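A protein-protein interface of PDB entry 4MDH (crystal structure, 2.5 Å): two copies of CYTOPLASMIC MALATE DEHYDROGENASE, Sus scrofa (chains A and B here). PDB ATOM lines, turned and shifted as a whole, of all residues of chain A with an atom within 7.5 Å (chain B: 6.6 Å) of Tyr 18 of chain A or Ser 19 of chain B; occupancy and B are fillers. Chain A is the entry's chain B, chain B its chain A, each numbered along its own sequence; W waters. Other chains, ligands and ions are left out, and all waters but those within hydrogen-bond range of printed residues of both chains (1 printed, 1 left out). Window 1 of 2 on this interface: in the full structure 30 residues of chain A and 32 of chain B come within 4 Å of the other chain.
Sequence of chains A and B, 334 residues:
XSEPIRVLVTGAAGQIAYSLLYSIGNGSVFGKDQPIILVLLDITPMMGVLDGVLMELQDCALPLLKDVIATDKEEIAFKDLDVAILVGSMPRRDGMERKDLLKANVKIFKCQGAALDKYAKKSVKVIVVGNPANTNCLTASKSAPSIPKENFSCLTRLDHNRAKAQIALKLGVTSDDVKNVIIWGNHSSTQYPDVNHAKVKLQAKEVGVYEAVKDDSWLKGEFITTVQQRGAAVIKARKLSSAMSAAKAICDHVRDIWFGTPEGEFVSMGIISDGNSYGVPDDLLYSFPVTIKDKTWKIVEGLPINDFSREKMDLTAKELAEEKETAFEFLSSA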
ATOM      1  N   VAL A   9       9.917 -33.404   2.267  1.00  0.00           N
ATOM      2  CA  VAL A   9       9.874 -32.923   0.901  1.00  0.00           C
ATOM      3  C   VAL A   9      11.310 -32.602   0.476  1.00  0.00           C
ATOM      4  O   VAL A   9      11.928 -31.658   0.944  1.00  0.00           O
ATOM      5  CB  VAL A   9       8.964 -31.669   0.639  1.00  0.00           C
ATOM      6  CG1 VAL A   9       9.041 -31.227  -0.823  1.00  0.00           C
ATOM      7  CG2 VAL A   9       7.503 -31.848   1.054  1.00  0.00           C
ATOM      8  N   GLY A  11      14.140 -31.518  -2.522  1.00  0.00           N
ATOM      9  CA  GLY A  11      14.149 -30.451  -3.540  1.00  0.00           C
ATOM     10  C   GLY A  11      13.499 -29.165  -3.027  1.00  0.00           C
ATOM     11  O   GLY A  11      13.300 -28.224  -3.774  1.00  0.00           O
ATOM     12  N   ALA A  12      13.205 -29.165  -1.711  1.00  0.00           N
ATOM     13  CA  ALA A  12      12.511 -28.137  -0.939  1.00  0.00           C
ATOM     14  C   ALA A  12      12.875 -26.637  -1.130  1.00  0.00           C
ATOM     15  O   ALA A  12      12.161 -25.739  -0.688  1.00  0.00           O
ATOM     16  CB  ALA A  12      12.300 -28.560   0.490  1.00  0.00           C
ATOM     17  N   ALA A  13      13.945 -26.348  -1.852  1.00  0.00           N
ATOM     18  CA  ALA A  13      14.203 -24.998  -2.168  1.00  0.00           C
ATOM     19  C   ALA A  13      13.791 -24.703  -3.604  1.00  0.00           C
ATOM     20  O   ALA A  13      13.728 -23.555  -4.002  1.00  0.00           O
ATOM     21  CB  ALA A  13      15.589 -24.556  -1.810  1.00  0.00           C
ATOM     22  N   GLY A  14      13.408 -25.733  -4.353  1.00  0.00           N
ATOM     23  CA  GLY A  14      12.950 -25.576  -5.744  1.00  0.00           C
ATOM     24  C   GLY A  14      11.580 -24.907  -5.864  1.00  0.00           C
ATOM     25  O   GLY A  14      10.972 -24.479  -4.885  1.00  0.00           O
ATOM     26  N   GLN A  15      11.105 -24.845  -7.095  1.00  0.00           N
ATOM     27  CA  GLN A  15       9.825 -24.271  -7.472  1.00  0.00           C
ATOM     28  C   GLN A  15       8.574 -25.051  -7.136  1.00  0.00           C
ATOM     29  O   GLN A  15       7.653 -24.468  -6.618  1.00  0.00           O
ATOM     30  CB  GLN A  15       9.821 -23.887  -8.923  1.00  0.00           C
ATOM     31  CG  GLN A  15      11.164 -23.296  -9.210  1.00  0.00           C
ATOM     32  CD  GLN A  15      11.319 -23.151 -10.673  1.00  0.00           C
ATOM     33  OE1 GLN A  15      10.537 -22.396 -11.249  1.00  0.00           O
ATOM     34  NE2 GLN A  15      12.293 -23.864 -11.266  1.00  0.00           N
ATOM     35  N   ILE A  16       8.479 -26.304  -7.501  1.00  0.00           N
ATOM     36  CA  ILE A  16       7.333 -27.050  -7.114  1.00  0.00           C
ATOM     37  C   ILE A  16       7.173 -27.013  -5.578  1.00  0.00           C
ATOM     38  O   ILE A  16       6.069 -26.752  -5.085  1.00  0.00           O
ATOM     39  CB  ILE A  16       7.360 -28.485  -7.640  1.00  0.00           C
ATOM     40  CG1 ILE A  16       7.619 -28.507  -9.123  1.00  0.00           C
ATOM     41  CG2 ILE A  16       6.058 -29.227  -7.360  1.00  0.00           C
ATOM     42  CD1 ILE A  16       7.019 -29.755  -9.757  1.00  0.00           C
ATOM     43  N   ALA A  17       8.251 -27.246  -4.800  1.00  0.00           N
ATOM     44  CA  ALA A  17       8.151 -27.254  -3.331  1.00  0.00           C
ATOM     45  C   ALA A  17       7.578 -26.013  -2.729  1.00  0.00           C
ATOM     46  O   ALA A  17       6.811 -26.069  -1.801  1.00  0.00           O
ATOM     47  CB  ALA A  17       9.451 -27.522  -2.635  1.00  0.00           C
ATOM     48  N   TYR A  18       7.969 -24.877  -3.262  1.00  0.00           N
ATOM     49  CA  TYR A  18       7.471 -23.610  -2.803  1.00  0.00           C
ATOM     50  C   TYR A  18       5.947 -23.476  -2.930  1.00  0.00           C
ATOM     51  O   TYR A  18       5.324 -22.749  -2.186  1.00  0.00           O
ATOM     52  CB  TYR A  18       8.243 -22.491  -3.510  1.00  0.00           C
ATOM     53  CG  TYR A  18       8.074 -21.141  -2.863  1.00  0.00           C
ATOM     54  CD1 TYR A  18       8.720 -20.820  -1.659  1.00  0.00           C
ATOM     55  CD2 TYR A  18       7.226 -20.210  -3.441  1.00  0.00           C
ATOM     56  CE1 TYR A  18       8.546 -19.583  -1.043  1.00  0.00           C
ATOM     57  CE2 TYR A  18       7.055 -18.957  -2.854  1.00  0.00           C
ATOM     58  CZ  TYR A  18       7.714 -18.643  -1.672  1.00  0.00           C
ATOM     59  OH  TYR A  18       7.548 -17.411  -1.142  1.00  0.00           O
ATOM     60  N   SER A  19       5.335 -24.189  -3.862  1.00  0.00           N
ATOM     61  CA  SER A  19       3.883 -24.115  -4.038  1.00  0.00           C
ATOM     62  C   SER A  19       3.141 -25.191  -3.281  1.00  0.00           C
ATOM     63  O   SER A  19       1.949 -25.062  -2.970  1.00  0.00           O
ATOM     64  CB  SER A  19       3.460 -24.194  -5.484  1.00  0.00           C
ATOM     65  OG  SER A  19       3.874 -23.025  -6.161  1.00  0.00           O
ATOM     66  N   LEU A  20       3.897 -26.232  -2.994  1.00  0.00           N
ATOM     67  CA  LEU A  20       3.461 -27.472  -2.395  1.00  0.00           C
ATOM     68  C   LEU A  20       3.397 -27.442  -0.880  1.00  0.00           C
ATOM     69  O   LEU A  20       2.462 -27.957  -0.263  1.00  0.00           O
ATOM     70  CB  LEU A  20       4.408 -28.583  -2.888  1.00  0.00           C
ATOM     71  CG  LEU A  20       4.300 -29.864  -2.107  1.00  0.00           C
ATOM     72  CD1 LEU A  20       2.859 -30.329  -2.114  1.00  0.00           C
ATOM     73  CD2 LEU A  20       5.222 -30.922  -2.715  1.00  0.00           C
ATOM     74  N   LEU A  21       4.426 -26.858  -0.294  1.00  0.00           N
ATOM     75  CA  LEU A  21       4.545 -26.790   1.138  1.00  0.00           C
ATOM     76  C   LEU A  21       3.315 -26.201   1.814  1.00  0.00           C
ATOM     77  O   LEU A  21       2.838 -26.744   2.783  1.00  0.00           O
ATOM     78  CB  LEU A  21       5.828 -26.047   1.546  1.00  0.00           C
ATOM     79  CG  LEU A  21       7.057 -26.930   1.458  1.00  0.00           C
ATOM     80  CD1 LEU A  21       8.256 -26.216   2.080  1.00  0.00           C
ATOM     81  CD2 LEU A  21       6.760 -28.176   2.240  1.00  0.00           C
ATOM     82  N   TYR A  22       2.831 -25.064   1.320  1.00  0.00           N
ATOM     83  CA  TYR A  22       1.704 -24.347   1.874  1.00  0.00           C
ATOM     84  C   TYR A  22       0.519 -25.263   2.124  1.00  0.00           C
ATOM     85  O   TYR A  22      -0.014 -25.335   3.210  1.00  0.00           O
ATOM     86  CB  TYR A  22       1.248 -23.194   0.944  1.00  0.00           C
ATOM     87  CG  TYR A  22       0.038 -22.577   1.576  1.00  0.00           C
ATOM     88  CD1 TYR A  22       0.122 -22.196   2.911  1.00  0.00           C
ATOM     89  CD2 TYR A  22      -1.230 -22.587   0.983  1.00  0.00           C
ATOM     90  CE1 TYR A  22      -0.979 -21.756   3.636  1.00  0.00           C
ATOM     91  CE2 TYR A  22      -2.345 -22.108   1.681  1.00  0.00           C
ATOM     92  CZ  TYR A  22      -2.215 -21.695   3.010  1.00  0.00           C
ATOM     93  OH  TYR A  22      -3.311 -21.291   3.759  1.00  0.00           O
ATOM     94  N   SER A  23       0.160 -25.944   1.050  1.00  0.00           N
ATOM     95  CA  SER A  23      -0.919 -26.864   0.859  1.00  0.00           C
ATOM     96  C   SER A  23      -0.760 -28.078   1.716  1.00  0.00           C
ATOM     97  O   SER A  23      -1.762 -28.688   2.142  1.00  0.00           O
ATOM     98  CB  SER A  23      -0.963 -27.308  -0.593  1.00  0.00           C
ATOM     99  OG  SER A  23      -1.915 -26.559  -1.351  1.00  0.00           O
ATOM    100  N   VAL A  49      18.493 -20.101   1.288  1.00  0.00           N
ATOM    101  CA  VAL A  49      17.158 -20.053   0.719  1.00  0.00           C
ATOM    102  C   VAL A  49      16.201 -20.918   1.485  1.00  0.00           C
ATOM    103  O   VAL A  49      15.028 -20.620   1.550  1.00  0.00           O
ATOM    104  CB  VAL A  49      17.170 -20.613  -0.684  1.00  0.00           C
ATOM    105  CG1 VAL A  49      15.746 -20.881  -1.147  1.00  0.00           C
ATOM    106  CG2 VAL A  49      17.949 -19.685  -1.606  1.00  0.00           C
ATOM    107  N   GLY A  52      15.069 -19.267   4.597  1.00  0.00           N
ATOM    108  CA  GLY A  52      14.121 -18.231   4.178  1.00  0.00           C
ATOM    109  C   GLY A  52      12.712 -18.847   4.045  1.00  0.00           C
ATOM    110  O   GLY A  52      11.733 -18.343   4.609  1.00  0.00           O
ATOM    111  N   VAL A  53      12.666 -19.965   3.307  1.00  0.00           N
ATOM    112  CA  VAL A  53      11.486 -20.723   3.041  1.00  0.00           C
ATOM    113  C   VAL A  53      10.993 -21.317   4.314  1.00  0.00           C
ATOM    114  O   VAL A  53       9.832 -21.621   4.455  1.00  0.00           O
ATOM    115  CB  VAL A  53      11.744 -21.822   2.038  1.00  0.00           C
ATOM    116  CG1 VAL A  53      10.599 -22.806   2.047  1.00  0.00           C
ATOM    117  CG2 VAL A  53      11.958 -21.241   0.637  1.00  0.00           C
ATOM    118  N   LEU A  54      11.875 -21.490   5.267  1.00  0.00           N
ATOM    119  CA  LEU A  54      11.415 -22.000   6.547  1.00  0.00           C
ATOM    120  C   LEU A  54      10.754 -20.900   7.370  1.00  0.00           C
ATOM    121  O   LEU A  54       9.737 -21.112   8.050  1.00  0.00           O
ATOM    122  CB  LEU A  54      12.466 -22.777   7.387  1.00  0.00           C
ATOM    123  CG  LEU A  54      11.996 -22.914   8.839  1.00  0.00           C
ATOM    124  CD1 LEU A  54      12.397 -24.264   9.387  1.00  0.00           C
ATOM    125  CD2 LEU A  54      12.577 -21.792   9.687  1.00  0.00           C
ATOM    126  N   GLU A  56       9.141 -18.449   6.285  1.00  0.00           N
ATOM    127  CA  GLU A  56       7.887 -18.280   5.617  1.00  0.00           C
ATOM    128  C   GLU A  56       6.874 -19.339   5.969  1.00  0.00           C
ATOM    129  O   GLU A  56       5.680 -19.121   5.845  1.00  0.00           O
ATOM    130  CB  GLU A  56       8.122 -18.302   4.099  1.00  0.00           C
ATOM    131  CG  GLU A  56       8.561 -16.960   3.523  1.00  0.00           C
ATOM    132  CD  GLU A  56       7.931 -16.598   2.208  1.00  0.00           C
ATOM    133  OE1 GLU A  56       6.829 -16.130   2.092  1.00  0.00           O
ATOM    134  OE2 GLU A  56       8.732 -16.790   1.203  1.00  0.00           O
ATOM    135  N   ALA A 243       4.637 -25.061 -11.554  1.00  0.00           N
ATOM    136  CA  ALA A 243       4.478 -25.227 -10.119  1.00  0.00           C
ATOM    137  C   ALA A 243       3.083 -25.254  -9.468  1.00  0.00           C
ATOM    138  O   ALA A 243       2.766 -26.086  -8.591  1.00  0.00           O
ATOM    139  CB  ALA A 243       5.466 -24.359  -9.362  1.00  0.00           C
ATOM    140  N   MET A 244       2.241 -24.311  -9.806  1.00  0.00           N
ATOM    141  CA  MET A 244       0.942 -24.339  -9.165  1.00  0.00           C
ATOM    142  C   MET A 244       0.188 -25.631  -9.519  1.00  0.00           C
ATOM    143  O   MET A 244      -0.386 -26.306  -8.634  1.00  0.00           O
ATOM    144  CB  MET A 244       0.150 -23.054  -9.524  1.00  0.00           C
ATOM    145  CG  MET A 244      -1.341 -23.099  -9.239  1.00  0.00           C
ATOM    146  SD  MET A 244      -2.304 -21.996 -10.301  1.00  0.00           S
ATOM    147  CE  MET A 244      -1.149 -20.617 -10.454  1.00  0.00           C
ATOM    148  N   ALA A 247       2.073 -28.889  -8.152  1.00  0.00           N
ATOM    149  CA  ALA A 247       1.840 -29.032  -6.710  1.00  0.00           C
ATOM    150  C   ALA A 247       0.418 -29.577  -6.372  1.00  0.00           C
ATOM    151  O   ALA A 247       0.214 -30.333  -5.419  1.00  0.00           O
ATOM    152  CB  ALA A 247       2.045 -27.680  -6.057  1.00  0.00           C
ATOM    153  N   GLY B  14       3.396 -11.942 -11.229  1.00  0.00           N
ATOM    154  CA  GLY B  14       4.522 -11.907 -10.343  1.00  0.00           C
ATOM    155  C   GLY B  14       4.461 -12.994  -9.299  1.00  0.00           C
ATOM    156  O   GLY B  14       3.576 -13.861  -9.321  1.00  0.00           O
ATOM    157  N   GLN B  15       5.419 -12.900  -8.389  1.00  0.00           N
ATOM    158  CA  GLN B  15       5.636 -13.827  -7.318  1.00  0.00           C
ATOM    159  C   GLN B  15       4.526 -14.003  -6.248  1.00  0.00           C
ATOM    160  O   GLN B  15       4.169 -15.109  -5.874  1.00  0.00           O
ATOM    161  CB  GLN B  15       7.058 -13.762  -6.743  1.00  0.00           C
ATOM    162  CG  GLN B  15       7.071 -14.446  -5.369  1.00  0.00           C
ATOM    163  CD  GLN B  15       8.374 -14.378  -4.588  1.00  0.00           C
ATOM    164  OE1 GLN B  15       9.017 -15.538  -4.523  1.00  0.00           O
ATOM    165  NE2 GLN B  15       8.753 -13.327  -4.002  1.00  0.00           N
ATOM    166  N   ILE B  16       3.956 -12.941  -5.708  1.00  0.00           N
ATOM    167  CA  ILE B  16       2.913 -13.135  -4.722  1.00  0.00           C
ATOM    168  C   ILE B  16       1.609 -13.618  -5.345  1.00  0.00           C
ATOM    169  O   ILE B  16       0.893 -14.418  -4.723  1.00  0.00           O
ATOM    170  CB  ILE B  16       2.676 -11.906  -3.890  1.00  0.00           C
ATOM    171  CG1 ILE B  16       3.887 -11.598  -3.062  1.00  0.00           C
ATOM    172  CG2 ILE B  16       1.436 -12.079  -3.005  1.00  0.00           C
ATOM    173  CD1 ILE B  16       3.618 -10.352  -2.249  1.00  0.00           C
ATOM    174  N   ALA B  17       1.286 -13.053  -6.526  1.00  0.00           N
ATOM    175  CA  ALA B  17       0.142 -13.422  -7.379  1.00  0.00           C
ATOM    176  C   ALA B  17       0.161 -14.889  -7.690  1.00  0.00           C
ATOM    177  O   ALA B  17      -0.890 -15.499  -7.799  1.00  0.00           O
ATOM    178  CB  ALA B  17       0.142 -12.700  -8.742  1.00  0.00           C
ATOM    179  N   TYR B  18       1.372 -15.416  -7.919  1.00  0.00           N
ATOM    180  CA  TYR B  18       1.527 -16.822  -8.273  1.00  0.00           C
ATOM    181  C   TYR B  18       1.177 -17.779  -7.114  1.00  0.00           C
ATOM    182  O   TYR B  18       0.611 -18.870  -7.339  1.00  0.00           O
ATOM    183  CB  TYR B  18       2.857 -17.123  -8.985  1.00  0.00           C
ATOM    184  CG  TYR B  18       2.914 -18.525  -9.586  1.00  0.00           C
ATOM    185  CD1 TYR B  18       2.299 -18.855 -10.788  1.00  0.00           C
ATOM    186  CD2 TYR B  18       3.619 -19.524  -8.944  1.00  0.00           C
ATOM    187  CE1 TYR B  18       2.396 -20.129 -11.347  1.00  0.00           C
ATOM    188  CE2 TYR B  18       3.786 -20.782  -9.508  1.00  0.00           C
ATOM    189  CZ  TYR B  18       3.141 -21.104 -10.693  1.00  0.00           C
ATOM    190  OH  TYR B  18       3.238 -22.386 -11.181  1.00  0.00           O
ATOM    191  N   SER B  19       1.465 -17.330  -5.859  1.00  0.00           N
ATOM    192  CA  SER B  19       1.112 -18.060  -4.664  1.00  0.00           C
ATOM    193  C   SER B  19      -0.321 -17.786  -4.217  1.00  0.00           C
ATOM    194  O   SER B  19      -1.002 -18.569  -3.578  1.00  0.00           O
ATOM    195  CB  SER B  19       2.085 -17.719  -3.568  1.00  0.00           C
ATOM    196  OG  SER B  19       3.375 -18.196  -3.909  1.00  0.00           O
ATOM    197  N   LEU B  20      -0.868 -16.704  -4.617  1.00  0.00           N
ATOM    198  CA  LEU B  20      -2.182 -16.379  -4.169  1.00  0.00           C
ATOM    199  C   LEU B  20      -3.373 -16.943  -5.027  1.00  0.00           C
ATOM    200  O   LEU B  20      -4.419 -17.331  -4.498  1.00  0.00           O
ATOM    201  CB  LEU B  20      -2.147 -14.834  -4.057  1.00  0.00           C
ATOM    202  CG  LEU B  20      -3.483 -14.188  -3.758  1.00  0.00           C
ATOM    203  CD1 LEU B  20      -3.856 -14.321  -2.264  1.00  0.00           C
ATOM    204  CD2 LEU B  20      -3.511 -12.745  -4.295  1.00  0.00           C
ATOM    205  N   LEU B  21      -3.251 -16.966  -6.357  1.00  0.00           N
ATOM    206  CA  LEU B  21      -4.314 -17.313  -7.319  1.00  0.00           C
ATOM    207  C   LEU B  21      -4.997 -18.651  -7.131  1.00  0.00           C
ATOM    208  O   LEU B  21      -6.191 -18.736  -7.445  1.00  0.00           O
ATOM    209  CB  LEU B  21      -3.863 -17.229  -8.785  1.00  0.00           C
ATOM    210  CG  LEU B  21      -3.658 -15.821  -9.300  1.00  0.00           C
ATOM    211  CD1 LEU B  21      -3.340 -15.866 -10.798  1.00  0.00           C
ATOM    212  CD2 LEU B  21      -4.926 -15.064  -9.072  1.00  0.00           C
ATOM    213  N   TYR B  22      -4.228 -19.685  -6.740  1.00  0.00           N
ATOM    214  CA  TYR B  22      -4.795 -20.995  -6.472  1.00  0.00           C
ATOM    215  C   TYR B  22      -5.775 -20.935  -5.327  1.00  0.00           C
ATOM    216  O   TYR B  22      -6.776 -21.637  -5.315  1.00  0.00           O
ATOM    217  CB  TYR B  22      -3.798 -22.168  -6.293  1.00  0.00           C
ATOM    218  CG  TYR B  22      -4.485 -23.474  -6.028  1.00  0.00           C
ATOM    219  CD1 TYR B  22      -5.193 -24.124  -7.045  1.00  0.00           C
ATOM    220  CD2 TYR B  22      -4.501 -24.077  -4.761  1.00  0.00           C
ATOM    221  CE1 TYR B  22      -5.903 -25.312  -6.795  1.00  0.00           C
ATOM    222  CE2 TYR B  22      -5.143 -25.288  -4.499  1.00  0.00           C
ATOM    223  CZ  TYR B  22      -5.844 -25.908  -5.535  1.00  0.00           C
ATOM    224  OH  TYR B  22      -6.493 -27.078  -5.333  1.00  0.00           O
ATOM    225  N   SER B  23      -5.514 -20.049  -4.362  1.00  0.00           N
ATOM    226  CA  SER B  23      -6.434 -19.890  -3.234  1.00  0.00           C
ATOM    227  C   SER B  23      -7.601 -18.912  -3.473  1.00  0.00           C
ATOM    228  O   SER B  23      -8.589 -18.906  -2.774  1.00  0.00           O
ATOM    229  CB  SER B  23      -5.797 -19.821  -1.867  1.00  0.00           C
ATOM    230  OG  SER B  23      -4.406 -20.109  -1.903  1.00  0.00           O
ATOM    231  N   ARG B 238      16.262 -15.892   0.988  1.00  0.00           N
ATOM    232  CA  ARG B 238      15.735 -16.273  -0.297  1.00  0.00           C
ATOM    233  C   ARG B 238      16.139 -15.336  -1.430  1.00  0.00           C
ATOM    234  O   ARG B 238      15.936 -15.631  -2.619  1.00  0.00           O
ATOM    235  CB  ARG B 238      14.202 -16.275  -0.217  1.00  0.00           C
ATOM    236  CG  ARG B 238      13.578 -17.490   0.471  1.00  0.00           C
ATOM    237  CD  ARG B 238      12.156 -17.881  -0.006  1.00  0.00           C
ATOM    238  NE  ARG B 238      11.364 -16.789  -0.565  1.00  0.00           N
ATOM    239  CZ  ARG B 238      11.139 -16.622  -1.883  1.00  0.00           C
ATOM    240  NH1 ARG B 238      11.605 -17.480  -2.807  1.00  0.00           N
ATOM    241  NH2 ARG B 238      10.439 -15.564  -2.285  1.00  0.00           N
ATOM    242  N   LEU B 240      14.671 -12.973  -2.299  1.00  0.00           N
ATOM    243  CA  LEU B 240      13.352 -12.540  -2.742  1.00  0.00           C
ATOM    244  C   LEU B 240      12.624 -12.175  -1.477  1.00  0.00           C
ATOM    245  O   LEU B 240      12.993 -12.685  -0.400  1.00  0.00           O
ATOM    246  CB  LEU B 240      12.533 -13.743  -3.293  1.00  0.00           C
ATOM    247  CG  LEU B 240      12.702 -14.092  -4.749  1.00  0.00           C
ATOM    248  CD1 LEU B 240      13.619 -13.110  -5.465  1.00  0.00           C
ATOM    249  CD2 LEU B 240      13.257 -15.500  -4.800  1.00  0.00           C
ATOM    250  N   SER B 241      11.569 -11.368  -1.600  1.00  0.00           N
ATOM    251  CA  SER B 241      10.745 -11.028  -0.427  1.00  0.00           C
ATOM    252  C   SER B 241       9.537 -11.957  -0.350  1.00  0.00           C
ATOM    253  O   SER B 241       9.261 -12.680  -1.296  1.00  0.00           O
ATOM    254  CB  SER B 241      10.374  -9.527  -0.318  1.00  0.00           C
ATOM    255  OG  SER B 241       9.765  -8.986  -1.507  1.00  0.00           O
ATOM    256  N   SER B 242       8.864 -11.943   0.802  1.00  0.00           N
ATOM    257  CA  SER B 242       7.642 -12.696   1.134  1.00  0.00           C
ATOM    258  C   SER B 242       6.765 -12.955  -0.076  1.00  0.00           C
ATOM    259  O   SER B 242       6.380 -12.003  -0.780  1.00  0.00           O
ATOM    260  CB  SER B 242       6.749 -11.848   2.035  1.00  0.00           C
ATOM    261  OG  SER B 242       7.304 -11.671   3.288  1.00  0.00           O
ATOM    262  N   ALA B 243       6.337 -14.198  -0.215  1.00  0.00           N
ATOM    263  CA  ALA B 243       5.455 -14.586  -1.259  1.00  0.00           C
ATOM    264  C   ALA B 243       4.465 -15.558  -0.710  1.00  0.00           C
ATOM    265  O   ALA B 243       3.304 -15.206  -0.529  1.00  0.00           O
ATOM    266  CB  ALA B 243       6.227 -15.078  -2.452  1.00  0.00           C
ATOM    267  N   MET B 244       4.939 -16.743  -0.367  1.00  0.00           N
ATOM    268  CA  MET B 244       4.146 -17.765   0.312  1.00  0.00           C
ATOM    269  C   MET B 244       3.378 -17.193   1.489  1.00  0.00           C
ATOM    270  O   MET B 244       2.165 -17.296   1.596  1.00  0.00           O
ATOM    271  CB  MET B 244       5.022 -18.927   0.860  1.00  0.00           C
ATOM    272  CG  MET B 244       4.261 -20.201   1.116  1.00  0.00           C
ATOM    273  SD  MET B 244       5.060 -21.276   2.338  1.00  0.00           S
ATOM    274  CE  MET B 244       6.379 -21.993   1.337  1.00  0.00           C
ATOM    275  N   SER B 245       4.128 -16.627   2.420  1.00  0.00           N
ATOM    276  CA  SER B 245       3.555 -16.052   3.610  1.00  0.00           C
ATOM    277  C   SER B 245       2.675 -14.808   3.340  1.00  0.00           C
ATOM    278  O   SER B 245       1.582 -14.644   3.914  1.00  0.00           O
ATOM    279  CB  SER B 245       4.635 -15.826   4.643  1.00  0.00           C
ATOM    280  OG  SER B 245       5.818 -15.437   3.996  1.00  0.00           O
ATOM    281  N   ALA B 247       1.109 -14.151   0.528  1.00  0.00           N
ATOM    282  CA  ALA B 247      -0.107 -14.591  -0.131  1.00  0.00           C
ATOM    283  C   ALA B 247      -1.160 -15.105   0.882  1.00  0.00           C
ATOM    284  O   ALA B 247      -2.340 -14.796   0.863  1.00  0.00           O
ATOM    285  CB  ALA B 247       0.286 -15.670  -1.124  1.00  0.00           C
ATOM    286  N   LYS B 248      -0.696 -15.935   1.763  1.00  0.00           N
ATOM    287  CA  LYS B 248      -1.450 -16.578   2.815  1.00  0.00           C
ATOM    288  C   LYS B 248      -2.209 -15.548   3.670  1.00  0.00           C
ATOM    289  O   LYS B 248      -3.345 -15.787   4.117  1.00  0.00           O
ATOM    290  CB  LYS B 248      -0.455 -17.481   3.602  1.00  0.00           C
ATOM    291  CG  LYS B 248      -0.863 -17.986   4.972  1.00  0.00           C
ATOM    292  CD  LYS B 248      -2.347 -18.200   5.096  1.00  0.00           C
ATOM    293  CE  LYS B 248      -2.674 -18.914   6.386  1.00  0.00           C
ATOM    294  NZ  LYS B 248      -2.415 -18.073   7.530  1.00  0.00           N
ATOM    295  N   CYS B 251      -5.137 -13.636   1.889  1.00  0.00           N
ATOM    296  CA  CYS B 251      -6.279 -14.506   2.085  1.00  0.00           C
ATOM    297  C   CYS B 251      -6.956 -14.239   3.398  1.00  0.00           C
ATOM    298  O   CYS B 251      -8.132 -13.990   3.430  1.00  0.00           O
ATOM    299  CB  CYS B 251      -5.908 -15.973   1.993  1.00  0.00           C
ATOM    300  SG  CYS B 251      -5.463 -16.341   0.309  1.00  0.00           S
HETATM  301  O   HOH W   1       3.795 -20.594  -2.551  1.00  0.00           O
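Of the 20 printed residues of chain B, 9 touch a printed residue of chain A. Hydrophobic or aromatic side chains of chain B that line the printed part of chain A: Tyr 18, Tyr 22, Ala 243 and Met 244. Among the printed residues, 16 pairs touch across the chains. Among the printed residues, Asp or Glu carboxylates within 4 Å of a Lys or Arg side-chain nitrogen of the other chain: Glu 56 of chain A with Arg 238 of chain B.
The guanidinium group (NH2) of Arg 238 of chain B sits at hydrogen-bond distance from the backbone carbonyl oxygen (O) of Ser 241 of chain B (3.3 Å).
OH of Tyr 18 of chain B sits at hydrogen-bond distance from N of Ala 243 of chain A (3.0 Å). The side-chain hydroxyl of Tyr 18 of chain B sits at hydrogen-bond distance from the backbone NH of Met 244 of chain A, 2.6 Å away. NE of Arg 238 of chain B lies within salt-bridge range of OE2 of Glu 56 of chain A. The backbone NH (N) of Ala 243 of chain B is in hydrogen-bond range of the side-chain carboxylate (OE1) of Glu 56 of chain A. The side-chain hydroxyl of Tyr 18 of chain A sits at hydrogen-bond distance from the backbone NH of Met 244 of chain B, at 2.8 Å. The backbone NH of Met 244 of chain B is in hydrogen-bond range of the side-chain carboxylate of Glu 56 of chain A (3.2 Å). The backbone NH of Ser 245 of chain B sits at hydrogen-bond distance from the side-chain carboxylate of Glu 56 of chain A (2.8 Å).
Water W1 lies within hydrogen-bond range of O of Tyr 18 of chain A (2.7 Å) and OG of Ser 19 of chain B (2.8 Å).
Met 244 of chain A touches Tyr 22 of chain B, but with the chains exchanged Tyr 22 of chain A does not touch Met 244 of chain B (4.3 Å). Of the 16 pairs that touch across the chains among the printed residues, 4 have their exchanged pair printed and touching as well.
Tyr 18 of chain A touches four residues of chain B. Of the printed residues of chain B, Gly 52 of chain A touches Arg 238 (3.8 Å). Of the printed residues of chain A, Tyr 18 of chain B touches Ala 243 (3.0 Å) and Met 244 (2.6 Å). Of the printed residues of chain A, Ser 245 of chain B touches Glu 56 (2.3 Å). The nearest residue of chain B that does not touch Tyr 18 of chain A is Gln 15 of chain B (4.1 Å). The nearest residue of chain A that does not touch Ser 19 of chain B is Ser 19 of chain A (5.4 Å). The nearest printed residue of chain A that does not touch Ser 242 of chain B is Tyr 18 of chain A (4.6 Å).
Among the printed residues, merely in contact across the chains: Tyr 18 of chain A with Ser 19 of chain B, Tyr 18 of chain A with Arg 238 of chain B, Tyr 18 of chain A with Ala 243 of chain B, Tyr 22 of chain A with Lys 248 of chain B, Val 49 of chain A with Arg 238 of chain B, Gly 52 of chain A with Arg 238 of chain B, Val 53 of chain A with Arg 238 of chain B, Glu 56 of chain A with Ser 242 of chain B and Met 244 of chain A with Tyr 22 of chain B.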
